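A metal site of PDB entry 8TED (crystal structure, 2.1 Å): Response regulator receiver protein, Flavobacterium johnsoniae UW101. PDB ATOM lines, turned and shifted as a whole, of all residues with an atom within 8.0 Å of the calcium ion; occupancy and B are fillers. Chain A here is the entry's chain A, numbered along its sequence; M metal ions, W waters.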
ATOM      1  N   VAL A  12      -4.745  19.361   6.920  1.00  0.00           N
ATOM      2  CA  VAL A  12      -3.570  20.060   6.318  1.00  0.00           C
ATOM      3  C   VAL A  12      -2.342  19.221   6.605  1.00  0.00           C
ATOM      4  O   VAL A  12      -2.005  19.056   7.811  1.00  0.00           O
ATOM      5  CB  VAL A  12      -3.358  21.475   6.904  1.00  0.00           C
ATOM      6  CG1 VAL A  12      -2.363  22.283   6.098  1.00  0.00           C
ATOM      7  CG2 VAL A  12      -4.663  22.216   7.054  1.00  0.00           C
ATOM      8  N   ASP A  13      -1.701  18.726   5.539  1.00  0.00           N
ATOM      9  CA  ASP A  13      -0.475  17.894   5.594  1.00  0.00           C
ATOM     10  C   ASP A  13       0.169  17.930   4.214  1.00  0.00           C
ATOM     11  O   ASP A  13      -0.559  17.823   3.228  1.00  0.00           O
ATOM     12  CB  ASP A  13      -0.789  16.461   6.039  1.00  0.00           C
ATOM     13  CG  ASP A  13       0.436  15.684   6.485  1.00  0.00           C
ATOM     14  OD1 ASP A  13       1.468  15.725   5.755  1.00  0.00           O
ATOM     15  OD2 ASP A  13       0.354  15.077   7.577  1.00  0.00           O
ATOM     16  N   ASP A  14       1.492  18.114   4.139  1.00  0.00           N
ATOM     17  CA  ASP A  14       2.187  18.216   2.821  1.00  0.00           C
ATOM     18  C   ASP A  14       2.130  16.853   2.134  1.00  0.00           C
ATOM     19  O   ASP A  14       2.258  16.836   0.899  1.00  0.00           O
ATOM     20  CB  ASP A  14       3.610  18.747   2.962  1.00  0.00           C
ATOM     21  CG  ASP A  14       4.500  17.879   3.825  1.00  0.00           C
ATOM     22  OD1 ASP A  14       5.212  17.045   3.266  1.00  0.00           O
ATOM     23  OD2 ASP A  14       4.435  17.982   5.048  1.00  0.00           O
ATOM     24  N   GLU A  15       1.900  15.778   2.898  1.00  0.00           N
ATOM     25  CA  GLU A  15       1.831  14.379   2.385  1.00  0.00           C
ATOM     26  C   GLU A  15       0.426  13.822   2.586  1.00  0.00           C
ATOM     27  O   GLU A  15       0.299  12.650   2.898  1.00  0.00           O
ATOM     28  CB  GLU A  15       2.884  13.544   3.117  1.00  0.00           C
ATOM     29  CG  GLU A  15       4.301  13.960   2.809  1.00  0.00           C
ATOM     30  CD  GLU A  15       5.378  13.278   3.632  1.00  0.00           C
ATOM     31  OE1 GLU A  15       5.113  12.884   4.778  1.00  0.00           O
ATOM     32  OE2 GLU A  15       6.501  13.166   3.118  1.00  0.00           O
ATOM     33  N   ILE A  16      -0.607  14.627   2.348  1.00  0.00           N
ATOM     34  CA  ILE A  16      -2.036  14.220   2.536  1.00  0.00           C
ATOM     35  C   ILE A  16      -2.355  13.059   1.570  1.00  0.00           C
ATOM     36  O   ILE A  16      -3.310  12.318   1.865  1.00  0.00           O
ATOM     37  CB  ILE A  16      -2.982  15.451   2.442  1.00  0.00           C
ATOM     38  CG1 ILE A  16      -4.378  15.192   2.993  1.00  0.00           C
ATOM     39  CG2 ILE A  16      -3.064  16.039   1.038  1.00  0.00           C
ATOM     40  CD1 ILE A  16      -4.411  14.442   4.306  1.00  0.00           C
ATOM     41  N   ASN A  37      -2.693  20.757   1.096  1.00  0.00           N
ATOM     42  CA  ASN A  37      -1.275  20.312   1.193  1.00  0.00           C
ATOM     43  C   ASN A  37      -0.405  21.441   1.731  1.00  0.00           C
ATOM     44  O   ASN A  37       0.809  21.185   1.886  1.00  0.00           O
ATOM     45  CB  ASN A  37      -0.770  19.695  -0.104  1.00  0.00           C
ATOM     46  CG  ASN A  37      -0.707  20.681  -1.258  1.00  0.00           C
ATOM     47  OD1 ASN A  37      -0.654  21.882  -1.048  1.00  0.00           O
ATOM     48  ND2 ASN A  37      -0.730  20.170  -2.465  1.00  0.00           N
ATOM     49  N   ASP A  57      -0.436  18.991  10.345  1.00  0.00           N
ATOM     50  CA  ASP A  57       0.949  18.477  10.490  1.00  0.00           C
ATOM     51  C   ASP A  57       1.826  19.611  11.016  1.00  0.00           C
ATOM     52  O   ASP A  57       1.504  20.763  10.709  1.00  0.00           O
ATOM     53  CB  ASP A  57       1.411  17.918   9.145  1.00  0.00           C
ATOM     54  CG  ASP A  57       2.807  17.298   9.152  1.00  0.00           C
ATOM     55  OD1 ASP A  57       3.295  16.819  10.220  1.00  0.00           O
ATOM     56  OD2 ASP A  57       3.367  17.271   8.067  1.00  0.00           O
ATOM     57  N   GLU A  58       2.890  19.335  11.765  1.00  0.00           N
ATOM     58  CA  GLU A  58       3.823  20.400  12.217  1.00  0.00           C
ATOM     59  C   GLU A  58       4.800  20.739  11.078  1.00  0.00           C
ATOM     60  O   GLU A  58       4.853  21.902  10.705  1.00  0.00           O
ATOM     61  CB  GLU A  58       4.573  20.064  13.500  1.00  0.00           C
ATOM     62  CG  GLU A  58       5.734  21.052  13.796  1.00  0.00           C
ATOM     63  CD  GLU A  58       5.421  22.551  13.817  1.00  0.00           C
ATOM     64  OE1 GLU A  58       4.248  22.939  13.611  1.00  0.00           O
ATOM     65  OE2 GLU A  58       6.335  23.340  14.100  1.00  0.00           O
ATOM     66  N   ASN A  59       5.559  19.780  10.559  1.00  0.00           N
ATOM     67  CA  ASN A  59       6.682  20.084   9.616  1.00  0.00           C
ATOM     68  C   ASN A  59       6.112  20.078   8.193  1.00  0.00           C
ATOM     69  O   ASN A  59       5.686  18.997   7.731  1.00  0.00           O
ATOM     70  CB  ASN A  59       7.912  19.179   9.794  1.00  0.00           C
ATOM     71  CG  ASN A  59       8.772  19.596  10.975  1.00  0.00           C
ATOM     72  OD1 ASN A  59       8.973  20.781  11.228  1.00  0.00           O
ATOM     73  ND2 ASN A  59       9.294  18.622  11.705  1.00  0.00           N
ATOM     74  N   MET A  60       6.083  21.258   7.577  1.00  0.00           N
ATOM     75  CA  MET A  60       5.632  21.489   6.181  1.00  0.00           C
ATOM     76  C   MET A  60       6.540  22.544   5.517  1.00  0.00           C
ATOM     77  O   MET A  60       7.106  23.410   6.182  1.00  0.00           O
ATOM     78  CB  MET A  60       4.172  21.941   6.159  1.00  0.00           C
ATOM     79  CG  MET A  60       3.166  20.870   6.573  1.00  0.00           C
ATOM     80  SD  MET A  60       1.389  21.391   6.375  1.00  0.00           S
ATOM     81  CE  MET A  60       1.262  22.618   7.664  1.00  0.00           C
ATOM     82  N   PRO A  61       6.765  22.449   4.193  1.00  0.00           N
ATOM     83  CA  PRO A  61       7.758  23.287   3.507  1.00  0.00           C
ATOM     84  C   PRO A  61       7.545  24.795   3.687  1.00  0.00           C
ATOM     85  O   PRO A  61       8.504  25.494   3.968  1.00  0.00           O
ATOM     86  CB  PRO A  61       7.577  22.947   2.020  1.00  0.00           C
ATOM     87  CG  PRO A  61       6.930  21.583   2.019  1.00  0.00           C
ATOM     88  CD  PRO A  61       6.110  21.501   3.301  1.00  0.00           C
ATOM     89  N   ILE A  84      -1.300  16.403  14.157  1.00  0.00           N
ATOM     90  CA  ILE A  84      -1.026  14.989  13.744  1.00  0.00           C
ATOM     91  C   ILE A  84       0.273  14.985  12.943  1.00  0.00           C
ATOM     92  O   ILE A  84       0.248  15.458  11.768  1.00  0.00           O
ATOM     93  CB  ILE A  84      -2.199  14.399  12.941  1.00  0.00           C
ATOM     94  CG1 ILE A  84      -3.525  14.530  13.691  1.00  0.00           C
ATOM     95  CG2 ILE A  84      -1.914  12.955  12.548  1.00  0.00           C
ATOM     96  CD1 ILE A  84      -4.729  13.882  12.994  1.00  0.00           C
ATOM     97  N   THR A  85       1.356  14.468  13.527  1.00  0.00           N
ATOM     98  CA  THR A  85       2.749  14.789  13.135  1.00  0.00           C
ATOM     99  C   THR A  85       3.719  13.668  13.544  1.00  0.00           C
ATOM    100  O   THR A  85       3.430  12.949  14.524  1.00  0.00           O
ATOM    101  CB  THR A  85       3.159  16.099  13.812  1.00  0.00           C
ATOM    102  OG1 THR A  85       4.497  16.444  13.476  1.00  0.00           O
ATOM    103  CG2 THR A  85       3.118  16.019  15.322  1.00  0.00           C
ATOM    104  N   LYS A  86       4.867  13.590  12.854  1.00  0.00           N
ATOM    105  CA  LYS A  86       5.966  12.623  13.172  1.00  0.00           C
ATOM    106  C   LYS A  86       6.755  13.173  14.356  1.00  0.00           C
ATOM    107  O   LYS A  86       7.401  12.384  15.014  1.00  0.00           O
ATOM    108  CB  LYS A  86       6.878  12.348  11.974  1.00  0.00           C
ATOM    109  CG  LYS A  86       6.284  11.565  10.815  1.00  0.00           C
ATOM    110  CD  LYS A  86       6.276  10.037  10.995  1.00  0.00           C
ATOM    111  CE  LYS A  86       5.604   9.288   9.855  1.00  0.00           C
ATOM    112  NZ  LYS A  86       5.302   7.866  10.178  1.00  0.00           N
ATOM    113  N   SER A  87       6.667  14.472  14.660  1.00  0.00           N
ATOM    114  CA  SER A  87       7.521  15.162  15.659  1.00  0.00           C
ATOM    115  C   SER A  87       7.280  14.598  17.061  1.00  0.00           C
ATOM    116  O   SER A  87       6.121  14.560  17.504  1.00  0.00           O
ATOM    117  CB  SER A  87       7.243  16.649  15.626  1.00  0.00           C
ATOM    118  OG  SER A  87       7.100  17.103  14.285  1.00  0.00           O
ATOM    119  N   LYS A 107       2.467  10.326  14.710  1.00  0.00           N
ATOM    120  CA  LYS A 107       2.502   9.377  13.573  1.00  0.00           C
ATOM    121  C   LYS A 107       3.546   8.295  13.841  1.00  0.00           C
ATOM    122  O   LYS A 107       4.559   8.591  14.483  1.00  0.00           O
ATOM    123  CB  LYS A 107       2.854  10.089  12.263  1.00  0.00           C
ATOM    124  CG  LYS A 107       1.791  10.971  11.662  1.00  0.00           C
ATOM    125  CD  LYS A 107       2.257  11.577  10.353  1.00  0.00           C
ATOM    126  CE  LYS A 107       1.253  12.565   9.792  1.00  0.00           C
ATOM    127  NZ  LYS A 107       1.787  13.174   8.555  1.00  0.00           N
HETATM  128 CA    CA M   1       5.319  17.052   6.832  1.00  0.00          CA
HETATM  129  O   HOH W   1       4.016  15.257   6.261  1.00  0.00           O
HETATM  130  O   HOH W   2       7.147  16.130   5.326  1.00  0.00           O
HETATM  131  O   HOH W   3       6.728  15.758   8.465  1.00  0.00           O
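The calcium ion is bound by O of Asn 59 (2.2 Å).
OD2 of Asp 14 is bound to the calcium ion (2.2 Å).
Water W1 is bound to the calcium ion, at 2.3 Å.
OD2 of Asp 57 is bound to the calcium ion (2.3 Å).
The calcium ion is bound by water W3 (2.5 Å).
The calcium ion is bound by water W2 (2.5 Å).
Three residues have an atom within 4 Å of the calcium ion: Asp 14, Asp 57 and Asn 59.
The nearest printed residue that does not touch the calcium ion is Asp 13 (4.2 Å).
Water W1 lies within hydrogen-bond range of the side-chain carboxylate of Asp 13 (2.6 Å) and the side-chain carboxylate of Glu 15 (3.0 Å).
OG1 of Thr 85 is in hydrogen-bond range of OD1 of Asp 57, 3.5 Å away.
N of Asp 57 is in hydrogen-bond range of O of Val 12, 3.0 Å away.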
